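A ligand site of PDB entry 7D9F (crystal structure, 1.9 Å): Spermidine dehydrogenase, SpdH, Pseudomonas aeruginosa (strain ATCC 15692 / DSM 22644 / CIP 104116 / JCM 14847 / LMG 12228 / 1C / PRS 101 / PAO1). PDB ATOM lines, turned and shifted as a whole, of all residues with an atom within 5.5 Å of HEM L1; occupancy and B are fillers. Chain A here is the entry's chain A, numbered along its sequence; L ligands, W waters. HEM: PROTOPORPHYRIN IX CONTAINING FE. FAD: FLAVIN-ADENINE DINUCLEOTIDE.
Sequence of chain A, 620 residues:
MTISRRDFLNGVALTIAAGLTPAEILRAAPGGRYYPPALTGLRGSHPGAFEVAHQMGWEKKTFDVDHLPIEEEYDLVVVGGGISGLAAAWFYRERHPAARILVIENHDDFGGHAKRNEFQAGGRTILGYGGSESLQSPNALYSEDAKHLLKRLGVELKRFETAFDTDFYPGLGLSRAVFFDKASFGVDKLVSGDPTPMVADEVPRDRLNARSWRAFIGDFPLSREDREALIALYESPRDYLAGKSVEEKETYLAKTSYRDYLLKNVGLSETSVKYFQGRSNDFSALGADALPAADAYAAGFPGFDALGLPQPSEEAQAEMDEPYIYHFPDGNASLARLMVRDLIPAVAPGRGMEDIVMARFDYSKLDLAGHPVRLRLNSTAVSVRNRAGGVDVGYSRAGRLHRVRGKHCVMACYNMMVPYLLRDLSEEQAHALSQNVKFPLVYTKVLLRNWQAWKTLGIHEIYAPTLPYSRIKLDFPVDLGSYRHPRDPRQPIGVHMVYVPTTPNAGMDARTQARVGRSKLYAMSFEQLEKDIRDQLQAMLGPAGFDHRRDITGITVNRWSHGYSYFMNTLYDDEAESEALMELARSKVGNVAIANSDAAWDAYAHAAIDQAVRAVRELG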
ATOM      1  N   SER A  45      20.186  10.608 -20.371  1.00  0.00           N
ATOM      2  CA  SER A  45      21.385  11.017 -19.642  1.00  0.00           C
ATOM      3  C   SER A  45      21.092  10.879 -18.150  1.00  0.00           C
ATOM      4  O   SER A  45      20.636  11.799 -17.473  1.00  0.00           O
ATOM      5  CB  SER A  45      21.793  12.430 -20.028  1.00  0.00           C
ATOM      6  OG  SER A  45      22.272  12.402 -21.365  1.00  0.00           O
ATOM      7  N   ALA A  49      26.102   9.707 -15.538  1.00  0.00           N
ATOM      8  CA  ALA A  49      26.631   9.853 -16.895  1.00  0.00           C
ATOM      9  C   ALA A  49      27.329  11.189 -17.118  1.00  0.00           C
ATOM     10  O   ALA A  49      28.209  11.267 -17.976  1.00  0.00           O
ATOM     11  CB  ALA A  49      25.510   9.682 -17.925  1.00  0.00           C
ATOM     12  N   PHE A  50      26.976  12.210 -16.348  1.00  0.00           N
ATOM     13  CA  PHE A  50      27.339  13.585 -16.668  1.00  0.00           C
ATOM     14  C   PHE A  50      28.154  14.291 -15.594  1.00  0.00           C
ATOM     15  O   PHE A  50      28.573  15.432 -15.814  1.00  0.00           O
ATOM     16  CB  PHE A  50      26.060  14.395 -16.931  1.00  0.00           C
ATOM     17  CG  PHE A  50      25.102  14.375 -15.781  1.00  0.00           C
ATOM     18  CD1 PHE A  50      24.122  13.378 -15.678  1.00  0.00           C
ATOM     19  CD2 PHE A  50      25.190  15.334 -14.771  1.00  0.00           C
ATOM     20  CE1 PHE A  50      23.252  13.360 -14.598  1.00  0.00           C
ATOM     21  CE2 PHE A  50      24.310  15.311 -13.683  1.00  0.00           C
ATOM     22  CZ  PHE A  50      23.341  14.324 -13.597  1.00  0.00           C
ATOM     23  N   ALA A  53      31.629  15.350 -16.626  1.00  0.00           N
ATOM     24  CA  ALA A  53      31.468  16.340 -17.687  1.00  0.00           C
ATOM     25  C   ALA A  53      31.096  17.700 -17.129  1.00  0.00           C
ATOM     26  O   ALA A  53      31.584  18.729 -17.625  1.00  0.00           O
ATOM     27  CB  ALA A  53      30.394  15.871 -18.673  1.00  0.00           C
ATOM     28  N   HIS A  54      30.229  17.736 -16.111  1.00  0.00           N
ATOM     29  CA  HIS A  54      29.847  19.015 -15.505  1.00  0.00           C
ATOM     30  C   HIS A  54      30.934  19.583 -14.603  1.00  0.00           C
ATOM     31  O   HIS A  54      31.023  20.809 -14.469  1.00  0.00           O
ATOM     32  CB  HIS A  54      28.557  18.868 -14.726  1.00  0.00           C
ATOM     33  CG  HIS A  54      27.344  18.874 -15.594  1.00  0.00           C
ATOM     34  ND1 HIS A  54      26.065  18.758 -15.102  1.00  0.00           N
ATOM     35  CD2 HIS A  54      27.227  19.010 -16.939  1.00  0.00           C
ATOM     36  CE1 HIS A  54      25.208  18.807 -16.100  1.00  0.00           C
ATOM     37  NE2 HIS A  54      25.880  18.968 -17.224  1.00  0.00           N
ATOM     38  N   GLY A  57      32.648  21.347 -17.350  1.00  0.00           N
ATOM     39  CA  GLY A  57      31.855  22.360 -18.011  1.00  0.00           C
ATOM     40  C   GLY A  57      31.338  23.438 -17.079  1.00  0.00           C
ATOM     41  O   GLY A  57      31.307  24.619 -17.449  1.00  0.00           O
ATOM     42  N   TRP A  58      30.924  23.058 -15.877  1.00  0.00           N
ATOM     43  CA  TRP A  58      30.374  24.044 -14.949  1.00  0.00           C
ATOM     44  C   TRP A  58      31.425  24.632 -14.006  1.00  0.00           C
ATOM     45  O   TRP A  58      31.443  25.844 -13.772  1.00  0.00           O
ATOM     46  CB  TRP A  58      29.261  23.425 -14.103  1.00  0.00           C
ATOM     47  CG  TRP A  58      28.045  23.032 -14.870  1.00  0.00           C
ATOM     48  CD1 TRP A  58      27.905  22.933 -16.223  1.00  0.00           C
ATOM     49  CD2 TRP A  58      26.775  22.666 -14.302  1.00  0.00           C
ATOM     50  NE1 TRP A  58      26.628  22.519 -16.534  1.00  0.00           N
ATOM     51  CE2 TRP A  58      25.922  22.360 -15.378  1.00  0.00           C
ATOM     52  CE3 TRP A  58      26.289  22.577 -13.003  1.00  0.00           C
ATOM     53  CZ2 TRP A  58      24.594  21.967 -15.177  1.00  0.00           C
ATOM     54  CZ3 TRP A  58      24.972  22.188 -12.809  1.00  0.00           C
ATOM     55  CH2 TRP A  58      24.149  21.889 -13.891  1.00  0.00           C
ATOM     56  N   LYS A  60      34.846  24.201 -14.269  1.00  0.00           N
ATOM     57  CA  LYS A  60      36.119  24.437 -14.959  1.00  0.00           C
ATOM     58  C   LYS A  60      37.263  23.703 -14.273  1.00  0.00           C
ATOM     59  O   LYS A  60      38.403  24.161 -14.289  1.00  0.00           O
ATOM     60  CB  LYS A  60      36.419  25.933 -15.065  1.00  0.00           C
ATOM     61  CG  LYS A  60      35.319  26.732 -15.736  1.00  0.00           C
ATOM     62  CD  LYS A  60      35.209  26.437 -17.231  1.00  0.00           C
ATOM     63  CE  LYS A  60      34.259  27.431 -17.915  1.00  0.00           C
ATOM     64  NZ  LYS A  60      32.988  26.775 -18.303  1.00  0.00           N
ATOM     65  N   ASN A 106      30.493   7.660 -22.006  1.00  0.00           N
ATOM     66  CA  ASN A 106      30.245   8.054 -20.623  1.00  0.00           C
ATOM     67  C   ASN A 106      28.923   7.554 -20.048  1.00  0.00           C
ATOM     68  O   ASN A 106      28.819   7.447 -18.818  1.00  0.00           O
ATOM     69  CB  ASN A 106      30.312   9.575 -20.476  1.00  0.00           C
ATOM     70  CG  ASN A 106      29.253  10.282 -21.269  1.00  0.00           C
ATOM     71  OD1 ASN A 106      29.014   9.984 -22.428  1.00  0.00           O
ATOM     72  ND2 ASN A 106      28.608  11.247 -20.640  1.00  0.00           N
ATOM     73  N   HIS A 107      27.921   7.230 -20.876  1.00  0.00           N
ATOM     74  CA  HIS A 107      26.686   6.638 -20.386  1.00  0.00           C
ATOM     75  C   HIS A 107      26.926   5.167 -19.988  1.00  0.00           C
ATOM     76  O   HIS A 107      27.968   4.586 -20.268  1.00  0.00           O
ATOM     77  CB  HIS A 107      25.583   6.687 -21.448  1.00  0.00           C
ATOM     78  CG  HIS A 107      25.029   8.059 -21.684  1.00  0.00           C
ATOM     79  ND1 HIS A 107      25.577   8.934 -22.603  1.00  0.00           N
ATOM     80  CD2 HIS A 107      23.979   8.713 -21.121  1.00  0.00           C
ATOM     81  CE1 HIS A 107      24.881  10.059 -22.604  1.00  0.00           C
ATOM     82  NE2 HIS A 107      23.918   9.953 -21.711  1.00  0.00           N
ATOM     83  N   TYR A 414      29.597  15.009 -28.141  1.00  0.00           N
ATOM     84  CA  TYR A 414      29.005  16.334 -28.292  1.00  0.00           C
ATOM     85  C   TYR A 414      30.073  17.355 -28.645  1.00  0.00           C
ATOM     86  O   TYR A 414      31.126  17.422 -28.011  1.00  0.00           O
ATOM     87  CB  TYR A 414      28.340  16.757 -26.984  1.00  0.00           C
ATOM     88  CG  TYR A 414      27.329  15.809 -26.375  1.00  0.00           C
ATOM     89  CD1 TYR A 414      26.584  14.924 -27.163  1.00  0.00           C
ATOM     90  CD2 TYR A 414      27.091  15.822 -25.016  1.00  0.00           C
ATOM     91  CE1 TYR A 414      25.637  14.097 -26.579  1.00  0.00           C
ATOM     92  CE2 TYR A 414      26.174  15.015 -24.441  1.00  0.00           C
ATOM     93  CZ  TYR A 414      25.435  14.158 -25.215  1.00  0.00           C
ATOM     94  OH  TYR A 414      24.512  13.359 -24.591  1.00  0.00           O
ATOM     95  N   MET A 416      30.191  20.619 -28.263  1.00  0.00           N
ATOM     96  CA  MET A 416      30.507  21.626 -27.245  1.00  0.00           C
ATOM     97  C   MET A 416      31.346  21.029 -26.098  1.00  0.00           C
ATOM     98  O   MET A 416      31.940  21.760 -25.311  1.00  0.00           O
ATOM     99  CB  MET A 416      29.236  22.291 -26.693  1.00  0.00           C
ATOM    100  CG  MET A 416      28.670  21.680 -25.429  1.00  0.00           C
ATOM    101  SD  MET A 416      27.681  20.027 -25.817  1.00  0.00           S
ATOM    102  CE  MET A 416      27.624  19.306 -23.995  1.00  0.00           C
ATOM    103  N   MET A 417      31.421  19.708 -26.020  1.00  0.00           N
ATOM    104  CA  MET A 417      32.318  19.039 -25.075  1.00  0.00           C
ATOM    105  C   MET A 417      33.797  19.097 -25.513  1.00  0.00           C
ATOM    106  O   MET A 417      34.699  19.096 -24.667  1.00  0.00           O
ATOM    107  CB  MET A 417      31.888  17.574 -24.907  1.00  0.00           C
ATOM    108  CG  MET A 417      32.777  16.747 -23.963  1.00  0.00           C
ATOM    109  SD  MET A 417      32.120  16.760 -22.121  1.00  0.00           S
ATOM    110  CE  MET A 417      33.328  18.152 -21.376  1.00  0.00           C
ATOM    111  N   TYR A 420      36.731  21.277 -23.850  1.00  0.00           N
ATOM    112  CA  TYR A 420      37.185  20.851 -22.536  1.00  0.00           C
ATOM    113  C   TYR A 420      38.141  19.681 -22.581  1.00  0.00           C
ATOM    114  O   TYR A 420      38.824  19.414 -21.595  1.00  0.00           O
ATOM    115  CB  TYR A 420      35.971  20.490 -21.668  1.00  0.00           C
ATOM    116  CG  TYR A 420      35.103  21.698 -21.451  1.00  0.00           C
ATOM    117  CD1 TYR A 420      35.461  22.676 -20.522  1.00  0.00           C
ATOM    118  CD2 TYR A 420      33.953  21.897 -22.194  1.00  0.00           C
ATOM    119  CE1 TYR A 420      34.693  23.806 -20.325  1.00  0.00           C
ATOM    120  CE2 TYR A 420      33.155  23.024 -22.000  1.00  0.00           C
ATOM    121  CZ  TYR A 420      33.535  23.982 -21.069  1.00  0.00           C
ATOM    122  OH  TYR A 420      32.777  25.103 -20.875  1.00  0.00           O
ATOM    123  N   SER A 434      31.880  25.591 -29.352  1.00  0.00           N
ATOM    124  CA  SER A 434      30.964  25.919 -28.258  1.00  0.00           C
ATOM    125  C   SER A 434      29.650  26.498 -28.766  1.00  0.00           C
ATOM    126  O   SER A 434      28.662  26.537 -28.015  1.00  0.00           O
ATOM    127  CB  SER A 434      31.641  26.911 -27.298  1.00  0.00           C
ATOM    128  OG  SER A 434      31.674  28.221 -27.867  1.00  0.00           O
ATOM    129  N   VAL A 437      24.973  24.618 -29.582  1.00  0.00           N
ATOM    130  CA  VAL A 437      24.196  24.499 -28.367  1.00  0.00           C
ATOM    131  C   VAL A 437      23.091  23.496 -28.670  1.00  0.00           C
ATOM    132  O   VAL A 437      22.219  23.764 -29.502  1.00  0.00           O
ATOM    133  CB  VAL A 437      23.644  25.860 -27.923  1.00  0.00           C
ATOM    134  CG1 VAL A 437      22.784  25.713 -26.672  1.00  0.00           C
ATOM    135  CG2 VAL A 437      24.777  26.869 -27.693  1.00  0.00           C
ATOM    136  N   ARG A 515      19.447  26.323 -23.648  1.00  0.00           N
ATOM    137  CA  ARG A 515      20.144  26.345 -22.357  1.00  0.00           C
ATOM    138  C   ARG A 515      19.157  26.444 -21.204  1.00  0.00           C
ATOM    139  O   ARG A 515      19.320  25.768 -20.186  1.00  0.00           O
ATOM    140  CB  ARG A 515      21.135  27.513 -22.304  1.00  0.00           C
ATOM    141  CG  ARG A 515      22.285  27.440 -23.307  1.00  0.00           C
ATOM    142  CD  ARG A 515      23.242  28.620 -23.061  1.00  0.00           C
ATOM    143  NE  ARG A 515      24.277  28.775 -24.080  1.00  0.00           N
ATOM    144  CZ  ARG A 515      24.293  29.747 -24.991  1.00  0.00           C
ATOM    145  NH1 ARG A 515      23.324  30.665 -25.030  1.00  0.00           N
ATOM    146  NH2 ARG A 515      25.288  29.810 -25.881  1.00  0.00           N
ATOM    147  N   ARG A 518      17.497  23.123 -20.512  1.00  0.00           N
ATOM    148  CA  ARG A 518      18.364  22.263 -19.711  1.00  0.00           C
ATOM    149  C   ARG A 518      18.328  22.663 -18.241  1.00  0.00           C
ATOM    150  O   ARG A 518      18.369  21.790 -17.354  1.00  0.00           O
ATOM    151  CB  ARG A 518      19.793  22.313 -20.236  1.00  0.00           C
ATOM    152  CG  ARG A 518      20.200  21.143 -21.033  1.00  0.00           C
ATOM    153  CD  ARG A 518      21.682  21.175 -21.394  1.00  0.00           C
ATOM    154  NE  ARG A 518      22.041  22.274 -22.292  1.00  0.00           N
ATOM    155  CZ  ARG A 518      21.742  22.312 -23.577  1.00  0.00           C
ATOM    156  NH1 ARG A 518      21.040  21.324 -24.145  1.00  0.00           N
ATOM    157  NH2 ARG A 518      22.127  23.346 -24.316  1.00  0.00           N
ATOM    158  N   SER A 519      18.293  23.962 -17.945  1.00  0.00           N
ATOM    159  CA  SER A 519      18.203  24.394 -16.553  1.00  0.00           C
ATOM    160  C   SER A 519      16.914  23.905 -15.925  1.00  0.00           C
ATOM    161  O   SER A 519      16.905  23.446 -14.776  1.00  0.00           O
ATOM    162  CB  SER A 519      18.303  25.921 -16.435  1.00  0.00           C
ATOM    163  OG  SER A 519      19.512  26.404 -16.982  1.00  0.00           O
ATOM    164  N   LEU A 521      15.208  21.196 -16.792  1.00  0.00           N
ATOM    165  CA  LEU A 521      15.323  19.752 -16.548  1.00  0.00           C
ATOM    166  C   LEU A 521      16.227  19.447 -15.362  1.00  0.00           C
ATOM    167  O   LEU A 521      15.977  18.494 -14.617  1.00  0.00           O
ATOM    168  CB  LEU A 521      15.860  19.033 -17.792  1.00  0.00           C
ATOM    169  CG  LEU A 521      14.936  18.956 -19.005  1.00  0.00           C
ATOM    170  CD1 LEU A 521      15.648  18.227 -20.184  1.00  0.00           C
ATOM    171  CD2 LEU A 521      13.610  18.267 -18.639  1.00  0.00           C
ATOM    172  N   TYR A 522      17.292  20.226 -15.186  1.00  0.00           N
ATOM    173  CA  TYR A 522      18.221  19.986 -14.077  1.00  0.00           C
ATOM    174  C   TYR A 522      17.537  20.197 -12.732  1.00  0.00           C
ATOM    175  O   TYR A 522      17.894  19.539 -11.745  1.00  0.00           O
ATOM    176  CB  TYR A 522      19.443  20.906 -14.211  1.00  0.00           C
ATOM    177  CG  TYR A 522      20.559  20.570 -13.270  1.00  0.00           C
ATOM    178  CD1 TYR A 522      21.328  19.423 -13.454  1.00  0.00           C
ATOM    179  CD2 TYR A 522      20.870  21.398 -12.186  1.00  0.00           C
ATOM    180  CE1 TYR A 522      22.362  19.095 -12.594  1.00  0.00           C
ATOM    181  CE2 TYR A 522      21.903  21.079 -11.322  1.00  0.00           C
ATOM    182  CZ  TYR A 522      22.645  19.929 -11.531  1.00  0.00           C
ATOM    183  OH  TYR A 522      23.670  19.605 -10.681  1.00  0.00           O
ATOM    184  N   ARG A 559      15.853  11.211 -20.531  1.00  0.00           N
ATOM    185  CA  ARG A 559      16.119  12.638 -20.394  1.00  0.00           C
ATOM    186  C   ARG A 559      17.315  13.007 -21.281  1.00  0.00           C
ATOM    187  O   ARG A 559      18.472  12.762 -20.920  1.00  0.00           O
ATOM    188  CB  ARG A 559      16.370  12.987 -18.927  1.00  0.00           C
ATOM    189  CG  ARG A 559      16.753  14.427 -18.673  1.00  0.00           C
ATOM    190  CD  ARG A 559      17.012  14.637 -17.197  1.00  0.00           C
ATOM    191  NE  ARG A 559      18.154  13.868 -16.733  1.00  0.00           N
ATOM    192  CZ  ARG A 559      18.525  13.808 -15.453  1.00  0.00           C
ATOM    193  NH1 ARG A 559      17.837  14.461 -14.524  1.00  0.00           N
ATOM    194  NH2 ARG A 559      19.586  13.086 -15.106  1.00  0.00           N
ATOM    195  N   SER A 561      19.068  15.765 -22.083  1.00  0.00           N
ATOM    196  CA  SER A 561      19.409  17.153 -21.780  1.00  0.00           C
ATOM    197  C   SER A 561      20.190  17.792 -22.911  1.00  0.00           C
ATOM    198  O   SER A 561      19.955  18.958 -23.260  1.00  0.00           O
ATOM    199  CB  SER A 561      20.173  17.210 -20.476  1.00  0.00           C
ATOM    200  OG  SER A 561      19.345  16.697 -19.453  1.00  0.00           O
ATOM    201  N   HIS A 562      21.127  17.059 -23.501  1.00  0.00           N
ATOM    202  CA  HIS A 562      21.805  17.462 -24.726  1.00  0.00           C
ATOM    203  C   HIS A 562      21.312  16.537 -25.841  1.00  0.00           C
ATOM    204  O   HIS A 562      21.879  15.464 -26.070  1.00  0.00           O
ATOM    205  CB  HIS A 562      23.295  17.380 -24.561  1.00  0.00           C
ATOM    206  CG  HIS A 562      23.802  18.244 -23.453  1.00  0.00           C
ATOM    207  ND1 HIS A 562      24.154  19.559 -23.636  1.00  0.00           N
ATOM    208  CD2 HIS A 562      23.994  17.978 -22.145  1.00  0.00           C
ATOM    209  CE1 HIS A 562      24.571  20.067 -22.491  1.00  0.00           C
ATOM    210  NE2 HIS A 562      24.482  19.126 -21.570  1.00  0.00           N
HETATM  211  CHA HEM L   1      26.076  22.386 -19.893  1.00  0.00           C
HETATM  212  CHB HEM L   1      28.135  18.073 -20.657  1.00  0.00           C
HETATM  213  CHC HEM L   1      24.043  15.959 -19.130  1.00  0.00           C
HETATM  214  CHD HEM L   1      22.239  20.255 -17.770  1.00  0.00           C
HETATM  215  C1A HEM L   1      27.007  21.420 -20.197  1.00  0.00           C
HETATM  216  C2A HEM L   1      28.380  21.642 -20.606  1.00  0.00           C
HETATM  217  C3A HEM L   1      28.952  20.457 -20.812  1.00  0.00           C
HETATM  218  C4A HEM L   1      27.957  19.428 -20.558  1.00  0.00           C
HETATM  219  CMA HEM L   1      30.403  20.209 -21.250  1.00  0.00           C
HETATM  220  CAA HEM L   1      29.075  23.026 -20.748  1.00  0.00           C
HETATM  221  CBA HEM L   1      28.689  23.663 -22.085  1.00  0.00           C
HETATM  222  CGA HEM L   1      29.658  24.771 -22.504  1.00  0.00           C
HETATM  223  O1A HEM L   1      30.354  25.352 -21.638  1.00  0.00           O
HETATM  224  O2A HEM L   1      29.726  25.086 -23.732  1.00  0.00           O
HETATM  225  C1B HEM L   1      27.175  17.118 -20.408  1.00  0.00           C
HETATM  226  C2B HEM L   1      27.227  15.718 -20.788  1.00  0.00           C
HETATM  227  C3B HEM L   1      26.086  15.145 -20.336  1.00  0.00           C
HETATM  228  C4B HEM L   1      25.285  16.166 -19.703  1.00  0.00           C
HETATM  229  CMB HEM L   1      28.419  15.074 -21.537  1.00  0.00           C
HETATM  230  CAB HEM L   1      25.534  13.698 -20.439  1.00  0.00           C
HETATM  231  CBB HEM L   1      26.108  12.741 -21.148  1.00  0.00           C
HETATM  232  C1C HEM L   1      23.232  16.916 -18.552  1.00  0.00           C
HETATM  233  C2C HEM L   1      22.024  16.658 -17.800  1.00  0.00           C
HETATM  234  C3C HEM L   1      21.501  17.846 -17.408  1.00  0.00           C
HETATM  235  C4C HEM L   1      22.385  18.880 -17.927  1.00  0.00           C
HETATM  236  CMC HEM L   1      21.531  15.221 -17.545  1.00  0.00           C
HETATM  237  CAC HEM L   1      20.234  18.167 -16.593  1.00  0.00           C
HETATM  238  CBC HEM L   1      19.369  17.246 -16.139  1.00  0.00           C
HETATM  239  C1D HEM L   1      23.123  21.209 -18.239  1.00  0.00           C
HETATM  240  C2D HEM L   1      22.969  22.642 -18.132  1.00  0.00           C
HETATM  241  C3D HEM L   1      24.025  23.231 -18.728  1.00  0.00           C
HETATM  242  C4D HEM L   1      24.884  22.187 -19.234  1.00  0.00           C
HETATM  243  CMD HEM L   1      21.779  23.362 -17.445  1.00  0.00           C
HETATM  244  CAD HEM L   1      24.320  24.731 -18.889  1.00  0.00           C
HETATM  245  CBD HEM L   1      23.652  25.267 -20.164  1.00  0.00           C
HETATM  246  CGD HEM L   1      24.461  24.971 -21.397  1.00  0.00           C
HETATM  247  O1D HEM L   1      24.011  24.139 -22.236  1.00  0.00           O
HETATM  248  O2D HEM L   1      25.568  25.556 -21.564  1.00  0.00           O
HETATM  249  NA  HEM L   1      26.779  20.059 -20.185  1.00  0.00           N
HETATM  250  NB  HEM L   1      25.973  17.362 -19.761  1.00  0.00           N
HETATM  251  NC  HEM L   1      23.414  18.283 -18.609  1.00  0.00           N
HETATM  252  ND  HEM L   1      24.309  20.968 -18.920  1.00  0.00           N
HETATM  253 FE   HEM L   1      25.136  19.174 -19.393  1.00  0.00          FE
HETATM  254  PA  FAD L   2      25.169  10.841 -29.715  1.00  0.00           P
HETATM  255  O1A FAD L   2      24.183   9.744 -29.933  1.00  0.00           O
HETATM  256  O2A FAD L   2      24.723  11.959 -28.802  1.00  0.00           O
HETATM  257  O5B FAD L   2      26.515  10.269 -29.213  1.00  0.00           O
HETATM  258  C5B FAD L   2      27.502  11.116 -28.582  1.00  0.00           C
HETATM  259  C4B FAD L   2      27.909  10.422 -27.306  1.00  0.00           C
HETATM  260  O4B FAD L   2      29.164  10.988 -26.808  1.00  0.00           O
HETATM  261  C3B FAD L   2      26.900  10.542 -26.156  1.00  0.00           C
HETATM  262  O3B FAD L   2      26.620   9.282 -25.569  1.00  0.00           O
HETATM  263  C2B FAD L   2      27.630  11.426 -25.145  1.00  0.00           C
HETATM  264  O2B FAD L   2      27.280  11.172 -23.795  1.00  0.00           O
HETATM  265  C1B FAD L   2      29.064  10.989 -25.410  1.00  0.00           C
HETATM  266  N9A FAD L   2      30.073  11.851 -24.804  1.00  0.00           N
HETATM  267  C8A FAD L   2      29.956  13.193 -24.526  1.00  0.00           C
HETATM  268  N7A FAD L   2      30.976  13.701 -23.885  1.00  0.00           N
HETATM  269  C5A FAD L   2      31.807  12.604 -23.678  1.00  0.00           C
HETATM  270  C6A FAD L   2      33.054  12.465 -23.032  1.00  0.00           C
HETATM  271  N6A FAD L   2      33.714  13.482 -22.465  1.00  0.00           N
HETATM  272  N1A FAD L   2      33.602  11.235 -22.994  1.00  0.00           N
HETATM  273  C2A FAD L   2      32.952  10.220 -23.560  1.00  0.00           C
HETATM  274  N3A FAD L   2      31.773  10.224 -24.190  1.00  0.00           N
HETATM  275  C4A FAD L   2      31.243  11.460 -24.213  1.00  0.00           C
HETATM  276  N1  FAD L   2      17.846  11.086 -35.856  1.00  0.00           N
HETATM  277  C2  FAD L   2      17.244  10.481 -36.919  1.00  0.00           C
HETATM  278  O2  FAD L   2      17.823  10.326 -37.997  1.00  0.00           O
HETATM  279  N3  FAD L   2      15.941  10.017 -36.796  1.00  0.00           N
HETATM  280  C4  FAD L   2      15.148  10.116 -35.662  1.00  0.00           C
HETATM  281  O4  FAD L   2      14.010   9.672 -35.673  1.00  0.00           O
HETATM  282  C4X FAD L   2      15.809  10.762 -34.529  1.00  0.00           C
HETATM  283  N5  FAD L   2      15.123  10.905 -33.387  1.00  0.00           N
HETATM  284  C5X FAD L   2      15.784  11.528 -32.322  1.00  0.00           C
HETATM  285  C6  FAD L   2      15.117  11.677 -31.097  1.00  0.00           C
HETATM  286  C7  FAD L   2      15.746  12.281 -30.000  1.00  0.00           C
HETATM  287  C7M FAD L   2      14.990  12.442 -28.708  1.00  0.00           C
HETATM  288  C8  FAD L   2      17.059  12.763 -30.135  1.00  0.00           C
HETATM  289  C8M FAD L   2      17.768  13.431 -28.988  1.00  0.00           C
HETATM  290  C9  FAD L   2      17.724  12.610 -31.351  1.00  0.00           C
HETATM  291  C9A FAD L   2      17.095  11.997 -32.431  1.00  0.00           C
HETATM  292  N10 FAD L   2      17.763  11.831 -33.665  1.00  0.00           N
HETATM  293  C10 FAD L   2      17.152  11.224 -34.729  1.00  0.00           C
HETATM  294  C1' FAD L   2      19.109  12.383 -33.863  1.00  0.00           C
HETATM  295  C2' FAD L   2      20.229  11.652 -33.145  1.00  0.00           C
HETATM  296  O2' FAD L   2      21.055  12.654 -32.527  1.00  0.00           O
HETATM  297  C3' FAD L   2      21.011  10.840 -34.180  1.00  0.00           C
HETATM  298  O3' FAD L   2      20.097   9.957 -34.812  1.00  0.00           O
HETATM  299  C4' FAD L   2      22.131   9.997 -33.575  1.00  0.00           C
HETATM  300  O4' FAD L   2      21.549   9.174 -32.566  1.00  0.00           O
HETATM  301  C5' FAD L   2      23.214  10.873 -33.000  1.00  0.00           C
HETATM  302  O5' FAD L   2      24.437  10.117 -32.905  1.00  0.00           O
HETATM  303  P   FAD L   2      25.786  10.818 -32.521  1.00  0.00           P
HETATM  304  O1P FAD L   2      25.989  11.973 -33.505  1.00  0.00           O
HETATM  305  O2P FAD L   2      26.836   9.804 -32.424  1.00  0.00           O
HETATM  306  O3P FAD L   2      25.544  11.509 -31.100  1.00  0.00           O
HETATM  307  O   HOH W   1      27.723  25.294 -25.572  1.00  0.00           O
HETATM  308  O   HOH W   2      25.380  23.701 -24.485  1.00  0.00           O
HETATM  309  O   HOH W   3      31.962  24.559 -25.126  1.00  0.00           O
HETATM  310  O   HOH W   4      29.950  26.244 -19.284  1.00  0.00           O
HETATM  311  O   HOH W   5      27.131  27.245 -19.607  1.00  0.00           O
HETATM  312  O   HOH W   6      26.321  26.904 -23.586  1.00  0.00           O
HETATM  313  O   HOH W   7      30.390  27.913 -23.708  1.00  0.00           O
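The guanidinium group of Arg 518 lies within salt-bridge range of an oxygen (O1D) of HEM L1, at 2.7 Å. A ring nitrogen (NE2) of His 562 is bound to an iron atom (FE) of HEM L1, at 2.3 Å. FE of HEM L1 is bound by NE2 of His 54 (2.3 Å). A ring nitrogen (ND1) of His 107 lies close to an oxygen (O2B) of FAD L2. The side-chain hydroxyl of Tyr 420 is in hydrogen-bond range of an oxygen (O1A) of HEM L1 (2.6 Å). The side-chain amide oxygen of Asn 106 sits at hydrogen-bond distance from an oxygen (O2B) of FAD L2 (2.5 Å). N6A of FAD L2 lies within hydrogen-bond range of SD of Met 417, at 3.7 Å.
O of Arg 515 lies within hydrogen-bond range of OG of Ser 519 (3.3 Å). NH1 of Arg 518 sits at hydrogen-bond distance from O of Ser 561. The side-chain amino group (NZ) of Lys 60 lies within hydrogen-bond range of the side-chain hydroxyl (OH) of Tyr 420 (3.1 Å). O of Ala 49 lies within hydrogen-bond range of ND2 of Asn 106, at 2.7 Å. OG of Ser 45 is in hydrogen-bond range of NE2 of His 107, at 3.0 Å. O of Arg 559 lies within hydrogen-bond range of N of Ser 45 (2.8 Å). O of Gly 57 is in hydrogen-bond range of NZ of Lys 60, 2.9 Å away.
Merely in contact with HEM L1: Asn 106, Ser 561, Trp 58, His 107, Phe 50, Met 416, Ser 45, Tyr 522, Arg 559, Ala 53, Ser 519, Met 417, Tyr 414, Arg 515, Leu 521 and Gly 57. Hydrophobic or aromatic side chains within 4 Å of HEM L1: Phe 50, Ala 53, His 54, Trp 58, His 107, Tyr 414, Met 416, Met 417, Tyr 420, Tyr 522 and His 562. Of the 24 residues printed, 20 come within 4 Å of HEM L1. The nearest printed residue that does not touch HEM L1 is Ala 49 (4.1 Å).
Water W6 lies within hydrogen-bond range of an oxygen (O2D) of HEM L1 and the guanidinium group (NE) of Arg 515. Water W4 lies within hydrogen-bond range of O1A of HEM L1 (2.5 Å), O of Gly 57 (2.8 Å), NZ of Lys 60 (3.2 Å) and OH of Tyr 420 (3.4 Å). Water W2 lies within hydrogen-bond range of an oxygen (O1D) of HEM L1 (2.7 Å) and the guanidinium group (NH2) of Arg 518 (3.3 Å). Water W3 bridges O2A of HEM L1 (2.7 Å) and O of Met 416 (2.8 Å). Water W1 bridges O2A of HEM L1 (2.7 Å) and O of Ser 434 (2.9 Å).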
